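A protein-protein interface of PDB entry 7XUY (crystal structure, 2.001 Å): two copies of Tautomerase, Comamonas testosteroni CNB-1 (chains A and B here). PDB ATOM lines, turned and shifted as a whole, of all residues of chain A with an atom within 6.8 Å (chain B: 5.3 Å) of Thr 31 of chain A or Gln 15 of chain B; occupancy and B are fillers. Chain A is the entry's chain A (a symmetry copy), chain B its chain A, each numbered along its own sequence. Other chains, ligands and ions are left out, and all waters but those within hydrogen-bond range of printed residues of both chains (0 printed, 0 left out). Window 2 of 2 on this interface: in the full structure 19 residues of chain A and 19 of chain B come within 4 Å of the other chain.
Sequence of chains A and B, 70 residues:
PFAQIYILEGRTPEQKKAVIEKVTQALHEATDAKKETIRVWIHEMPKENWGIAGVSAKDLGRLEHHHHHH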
ATOM      1  N   PRO A   1       2.717  26.930  22.044  1.00  0.00           N
ATOM      2  CA  PRO A   1       2.672  25.682  21.267  1.00  0.00           C
ATOM      3  C   PRO A   1       4.068  25.231  20.851  1.00  0.00           C
ATOM      4  O   PRO A   1       4.926  26.058  20.522  1.00  0.00           O
ATOM      5  CB  PRO A   1       1.816  26.047  20.052  1.00  0.00           C
ATOM      6  CG  PRO A   1       1.757  27.533  20.038  1.00  0.00           C
ATOM      7  CD  PRO A   1       1.871  27.972  21.457  1.00  0.00           C
ATOM      8  N   ALA A  26       3.748  28.744  10.882  1.00  0.00           N
ATOM      9  CA  ALA A  26       2.545  27.931  10.738  1.00  0.00           C
ATOM     10  C   ALA A  26       1.768  27.844  12.050  1.00  0.00           C
ATOM     11  O   ALA A  26       0.535  27.977  12.061  1.00  0.00           O
ATOM     12  CB  ALA A  26       2.931  26.531  10.256  1.00  0.00           C
ATOM     13  N   LEU A  27       2.468  27.637  13.165  1.00  0.00           N
ATOM     14  CA  LEU A  27       1.786  27.554  14.452  1.00  0.00           C
ATOM     15  C   LEU A  27       1.239  28.914  14.873  1.00  0.00           C
ATOM     16  O   LEU A  27       0.141  29.001  15.437  1.00  0.00           O
ATOM     17  CB  LEU A  27       2.735  27.002  15.516  1.00  0.00           C
ATOM     18  CG  LEU A  27       3.134  25.516  15.467  1.00  0.00           C
ATOM     19  CD1 LEU A  27       4.083  25.208  16.615  1.00  0.00           C
ATOM     20  CD2 LEU A  27       1.917  24.580  15.519  1.00  0.00           C
ATOM     21  N   HIS A  28       1.996  29.987  14.613  1.00  0.00           N
ATOM     22  CA  HIS A  28       1.499  31.334  14.891  1.00  0.00           C
ATOM     23  C   HIS A  28       0.201  31.610  14.145  1.00  0.00           C
ATOM     24  O   HIS A  28      -0.745  32.163  14.717  1.00  0.00           O
ATOM     25  CB  HIS A  28       2.551  32.380  14.520  1.00  0.00           C
ATOM     26  CG  HIS A  28       2.020  33.783  14.478  1.00  0.00           C
ATOM     27  ND1 HIS A  28       1.651  34.472  15.613  1.00  0.00           N
ATOM     28  CD2 HIS A  28       1.809  34.631  13.440  1.00  0.00           C
ATOM     29  CE1 HIS A  28       1.233  35.683  15.276  1.00  0.00           C
ATOM     30  NE2 HIS A  28       1.313  35.801  13.963  1.00  0.00           N
ATOM     31  N   GLU A  29       0.129  31.233  12.866  1.00  0.00           N
ATOM     32  CA  GLU A  29      -1.057  31.566  12.081  1.00  0.00           C
ATOM     33  C   GLU A  29      -2.235  30.664  12.419  1.00  0.00           C
ATOM     34  O   GLU A  29      -3.385  31.113  12.387  1.00  0.00           O
ATOM     35  CB  GLU A  29      -0.753  31.464  10.589  1.00  0.00           C
ATOM     36  CG  GLU A  29       0.277  32.452  10.097  1.00  0.00           C
ATOM     37  CD  GLU A  29       0.621  32.227   8.640  1.00  0.00           C
ATOM     38  OE1 GLU A  29       0.175  31.196   8.088  1.00  0.00           O
ATOM     39  OE2 GLU A  29       1.344  33.061   8.055  1.00  0.00           O
ATOM     40  N   ALA A  30      -1.967  29.400  12.744  1.00  0.00           N
ATOM     41  CA  ALA A  30      -3.033  28.440  13.008  1.00  0.00           C
ATOM     42  C   ALA A  30      -3.679  28.653  14.369  1.00  0.00           C
ATOM     43  O   ALA A  30      -4.867  28.367  14.535  1.00  0.00           O
ATOM     44  CB  ALA A  30      -2.483  27.013  12.923  1.00  0.00           C
ATOM     45  N   THR A  31      -2.914  29.120  15.351  1.00  0.00           N
ATOM     46  CA  THR A  31      -3.396  29.244  16.715  1.00  0.00           C
ATOM     47  C   THR A  31      -3.413  30.669  17.233  1.00  0.00           C
ATOM     48  O   THR A  31      -3.937  30.895  18.328  1.00  0.00           O
ATOM     49  CB  THR A  31      -2.527  28.423  17.680  1.00  0.00           C
ATOM     50  OG1 THR A  31      -1.260  29.077  17.822  1.00  0.00           O
ATOM     51  CG2 THR A  31      -2.316  27.008  17.176  1.00  0.00           C
ATOM     52  N   ASP A  32      -2.796  31.610  16.524  1.00  0.00           N
ATOM     53  CA  ASP A  32      -2.660  33.003  16.946  1.00  0.00           C
ATOM     54  C   ASP A  32      -1.835  33.154  18.219  1.00  0.00           C
ATOM     55  O   ASP A  32      -1.924  34.182  18.901  1.00  0.00           O
ATOM     56  CB  ASP A  32      -4.025  33.665  17.111  1.00  0.00           C
ATOM     57  CG  ASP A  32      -4.722  33.853  15.795  1.00  0.00           C
ATOM     58  OD1 ASP A  32      -5.904  33.457  15.690  1.00  0.00           O
ATOM     59  OD2 ASP A  32      -4.079  34.387  14.859  1.00  0.00           O
ATOM     60  N   ALA A  33      -1.033  32.146  18.543  1.00  0.00           N
ATOM     61  CA  ALA A  33      -0.134  32.235  19.680  1.00  0.00           C
ATOM     62  C   ALA A  33       0.974  33.230  19.397  1.00  0.00           C
ATOM     63  O   ALA A  33       1.476  33.323  18.274  1.00  0.00           O
ATOM     64  CB  ALA A  33       0.481  30.872  19.990  1.00  0.00           C
ATOM     65  N   LYS A  34       1.369  33.964  20.425  1.00  0.00           N
ATOM     66  CA  LYS A  34       2.499  34.862  20.274  1.00  0.00           C
ATOM     67  C   LYS A  34       3.750  34.068  19.916  1.00  0.00           C
ATOM     68  O   LYS A  34       4.010  32.993  20.466  1.00  0.00           O
ATOM     69  CB  LYS A  34       2.688  35.674  21.550  1.00  0.00           C
ATOM     70  CG  LYS A  34       1.882  36.946  21.500  1.00  0.00           C
ATOM     71  CD  LYS A  34       1.306  37.316  22.838  1.00  0.00           C
ATOM     72  CE  LYS A  34       2.337  38.006  23.719  1.00  0.00           C
ATOM     73  NZ  LYS A  34       2.242  37.549  25.167  1.00  0.00           N
ATOM     74  N   ILE A  38       6.370  30.183  21.087  1.00  0.00           N
ATOM     75  CA  ILE A  38       6.463  29.021  20.207  1.00  0.00           C
ATOM     76  C   ILE A  38       7.874  28.446  20.235  1.00  0.00           C
ATOM     77  O   ILE A  38       8.872  29.176  20.182  1.00  0.00           O
ATOM     78  CB  ILE A  38       6.035  29.408  18.784  1.00  0.00           C
ATOM     79  CG1 ILE A  38       4.621  29.999  18.841  1.00  0.00           C
ATOM     80  CG2 ILE A  38       6.106  28.205  17.868  1.00  0.00           C
ATOM     81  CD1 ILE A  38       4.094  30.526  17.521  1.00  0.00           C
ATOM     82  N   ILE B   7      -0.099  21.407  22.105  1.00  0.00           N
ATOM     83  CA  ILE B   7      -0.871  22.623  22.364  1.00  0.00           C
ATOM     84  C   ILE B   7      -1.677  22.420  23.637  1.00  0.00           C
ATOM     85  O   ILE B   7      -1.955  21.290  24.056  1.00  0.00           O
ATOM     86  CB  ILE B   7      -1.833  23.001  21.207  1.00  0.00           C
ATOM     87  CG1 ILE B   7      -2.827  21.861  20.943  1.00  0.00           C
ATOM     88  CG2 ILE B   7      -1.067  23.342  19.920  1.00  0.00           C
ATOM     89  CD1 ILE B   7      -3.917  22.196  19.909  1.00  0.00           C
ATOM     90  N   ARG B  11      -8.564  24.760  22.090  1.00  0.00           N
ATOM     91  CA  ARG B  11      -8.548  25.404  20.787  1.00  0.00           C
ATOM     92  C   ARG B  11      -9.636  24.842  19.888  1.00  0.00           C
ATOM     93  O   ARG B  11     -10.047  23.685  20.026  1.00  0.00           O
ATOM     94  CB  ARG B  11      -7.186  25.251  20.129  1.00  0.00           C
ATOM     95  CG  ARG B  11      -6.133  25.934  20.939  1.00  0.00           C
ATOM     96  CD  ARG B  11      -4.823  26.012  20.213  1.00  0.00           C
ATOM     97  NE  ARG B  11      -3.838  26.693  21.048  1.00  0.00           N
ATOM     98  CZ  ARG B  11      -3.829  28.001  21.283  1.00  0.00           C
ATOM     99  NH1 ARG B  11      -4.757  28.788  20.744  1.00  0.00           N
ATOM    100  NH2 ARG B  11      -2.886  28.521  22.059  1.00  0.00           N
ATOM    101  N   THR B  12     -10.099  25.679  18.957  1.00  0.00           N
ATOM    102  CA  THR B  12     -11.191  25.306  18.078  1.00  0.00           C
ATOM    103  C   THR B  12     -10.761  24.169  17.162  1.00  0.00           C
ATOM    104  O   THR B  12      -9.567  23.963  16.925  1.00  0.00           O
ATOM    105  CB  THR B  12     -11.632  26.497  17.224  1.00  0.00           C
ATOM    106  OG1 THR B  12     -10.627  26.769  16.243  1.00  0.00           O
ATOM    107  CG2 THR B  12     -11.833  27.734  18.076  1.00  0.00           C
ATOM    108  N   PRO B  13     -11.719  23.404  16.630  1.00  0.00           N
ATOM    109  CA  PRO B  13     -11.346  22.401  15.620  1.00  0.00           C
ATOM    110  C   PRO B  13     -10.778  23.022  14.356  1.00  0.00           C
ATOM    111  O   PRO B  13      -9.912  22.413  13.715  1.00  0.00           O
ATOM    112  CB  PRO B  13     -12.664  21.656  15.353  1.00  0.00           C
ATOM    113  CG  PRO B  13     -13.725  22.538  15.902  1.00  0.00           C
ATOM    114  CD  PRO B  13     -13.119  23.268  17.047  1.00  0.00           C
ATOM    115  N   GLU B  14     -11.215  24.234  14.003  1.00  0.00           N
ATOM    116  CA  GLU B  14     -10.647  24.921  12.849  1.00  0.00           C
ATOM    117  C   GLU B  14      -9.164  25.214  13.057  1.00  0.00           C
ATOM    118  O   GLU B  14      -8.354  25.059  12.133  1.00  0.00           O
ATOM    119  CB  GLU B  14     -11.419  26.213  12.575  1.00  0.00           C
ATOM    120  CG  GLU B  14     -12.890  26.019  12.218  1.00  0.00           C
ATOM    121  CD  GLU B  14     -13.794  25.768  13.427  1.00  0.00           C
ATOM    122  OE1 GLU B  14     -14.884  25.184  13.238  1.00  0.00           O
ATOM    123  OE2 GLU B  14     -13.414  26.138  14.561  1.00  0.00           O
ATOM    124  N   GLN B  15      -8.787  25.636  14.265  1.00  0.00           N
ATOM    125  CA  GLN B  15      -7.379  25.882  14.553  1.00  0.00           C
ATOM    126  C   GLN B  15      -6.565  24.593  14.485  1.00  0.00           C
ATOM    127  O   GLN B  15      -5.408  24.604  14.047  1.00  0.00           O
ATOM    128  CB  GLN B  15      -7.238  26.542  15.923  1.00  0.00           C
ATOM    129  CG  GLN B  15      -7.759  27.991  15.953  1.00  0.00           C
ATOM    130  CD  GLN B  15      -7.562  28.642  17.306  1.00  0.00           C
ATOM    131  OE1 GLN B  15      -7.706  27.991  18.341  1.00  0.00           O
ATOM    132  NE2 GLN B  15      -7.229  29.926  17.310  1.00  0.00           N
ATOM    133  N   LYS B  16      -7.146  23.470  14.907  1.00  0.00           N
ATOM    134  CA  LYS B  16      -6.379  22.230  14.874  1.00  0.00           C
ATOM    135  C   LYS B  16      -6.206  21.735  13.442  1.00  0.00           C
ATOM    136  O   LYS B  16      -5.116  21.290  13.067  1.00  0.00           O
ATOM    137  CB  LYS B  16      -7.034  21.181  15.776  1.00  0.00           C
ATOM    138  CG  LYS B  16      -6.671  21.387  17.272  1.00  0.00           C
ATOM    139  CD  LYS B  16      -7.398  20.412  18.177  1.00  0.00           C
ATOM    140  CE  LYS B  16      -8.690  21.016  18.705  1.00  0.00           C
ATOM    141  NZ  LYS B  16      -9.564  19.994  19.362  1.00  0.00           N
ATOM    142  N   LYS B  17      -7.256  21.840  12.619  1.00  0.00           N
ATOM    143  CA  LYS B  17      -7.115  21.536  11.195  1.00  0.00           C
ATOM    144  C   LYS B  17      -6.068  22.432  10.540  1.00  0.00           C
ATOM    145  O   LYS B  17      -5.226  21.958   9.769  1.00  0.00           O
ATOM    146  CB  LYS B  17      -8.471  21.671  10.496  1.00  0.00           C
ATOM    147  CG  LYS B  17      -8.484  21.306   9.015  1.00  0.00           C
ATOM    148  CD  LYS B  17      -9.912  21.187   8.503  1.00  0.00           C
ATOM    149  CE  LYS B  17      -9.938  20.693   7.065  1.00  0.00           C
ATOM    150  NZ  LYS B  17     -11.282  20.779   6.467  1.00  0.00           N
ATOM    151  N   ALA B  18      -6.079  23.728  10.865  1.00  0.00           N
ATOM    152  CA  ALA B  18      -5.057  24.641  10.355  1.00  0.00           C
ATOM    153  C   ALA B  18      -3.652  24.251  10.825  1.00  0.00           C
ATOM    154  O   ALA B  18      -2.680  24.391  10.069  1.00  0.00           O
ATOM    155  CB  ALA B  18      -5.384  26.065  10.784  1.00  0.00           C
ATOM    156  N   VAL B  19      -3.509  23.787  12.070  1.00  0.00           N
ATOM    157  CA  VAL B  19      -2.200  23.295  12.498  1.00  0.00           C
ATOM    158  C   VAL B  19      -1.733  22.193  11.557  1.00  0.00           C
ATOM    159  O   VAL B  19      -0.614  22.229  11.033  1.00  0.00           O
ATOM    160  CB  VAL B  19      -2.236  22.803  13.959  1.00  0.00           C
ATOM    161  CG1 VAL B  19      -0.954  22.007  14.286  1.00  0.00           C
ATOM    162  CG2 VAL B  19      -2.386  23.960  14.940  1.00  0.00           C
ATOM    163  N   ILE B  20      -2.598  21.211  11.306  1.00  0.00           N
ATOM    164  CA  ILE B  20      -2.229  20.097  10.440  1.00  0.00           C
ATOM    165  C   ILE B  20      -1.881  20.604   9.043  1.00  0.00           C
ATOM    166  O   ILE B  20      -0.859  20.221   8.459  1.00  0.00           O
ATOM    167  CB  ILE B  20      -3.364  19.054  10.405  1.00  0.00           C
ATOM    168  CG1 ILE B  20      -3.381  18.246  11.727  1.00  0.00           C
ATOM    169  CG2 ILE B  20      -3.199  18.121   9.207  1.00  0.00           C
ATOM    170  CD1 ILE B  20      -4.570  17.292  11.812  1.00  0.00           C
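No position is printed for both chains.
The guanidinium group (NH1) of Arg 11 of chain B lies within hydrogen-bond range of the backbone carbonyl oxygen (O) of Thr 31 of chain A (3.3 Å).
The backbone NH of Gln 15 of chain B sits at hydrogen-bond distance from the side-chain hydroxyl of Thr 12 of chain B (2.9 Å).
OG1 of Thr 31 of chain A is in hydrogen-bond range of O of Leu 27 of chain A.
OG1 of Thr 31 of chain A sits close to N of Ala 33 of chain A (3.2 Å).
Ile 7 of chain B touches Pro 1 of chain A (CG2 to CB, 3.96 Å).
Gln 15 of chain B touches Ala 30 of chain A (CG to O, 3.2 Å).
C of Ala 18 of chain B touches CB of Ala 30 of chain A (3.7 Å).
N of Val 19 of chain B touches CB of Ala 30 of chain A, at 3.5 Å.
Thr 31 of chain A touches Gln 15 of chain B (O to NE2, 3.6 Å).
Val 19 of chain B touches Thr 31 of chain A (CG2 to CG2, 3.8 Å).
Hydrophobic or aromatic side chains of chain A that line the printed part of chain B: Pro 1 and Ala 30.
Of the 11 printed residues of chain B, 5 touch a printed residue of chain A.
Printed residues of chain B that touch a printed residue of chain A: Ile 7, Arg 11, Gln 15, Ala 18 and Val 19.
Among the printed residues, no Asp or Glu carboxylate lies within 4 Å of a Lys or Arg side-chain nitrogen of the other chain.
Of chain B, only Arg 11 (3.3 Å), Gln 15 (3.6 Å) and Val 19 (3.8 Å) come within 4 Å of Thr 31 of chain A.
Gln 15 of chain B touches two residues of chain A.
Printed residues of chain A within 4 Å of Arg 11 of chain B: Thr 31 (3.3 Å).
Of the printed residues of chain B, Pro 1 of chain A touches Ile 7 (3.96 Å).
Of the printed residues of chain B, Ala 30 of chain A touches Gln 15, Ala 18 and Val 19.
Printed residues of chain A within 4 Å of Val 19 of chain B: Ala 30 and Thr 31.
The nearest residue of chain A that does not touch Gln 15 of chain B is Asp 32 of chain A (4.1 Å).
The nearest printed residue of chain A that does not touch Ala 18 of chain B is Ala 26 of chain A (5.2 Å).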
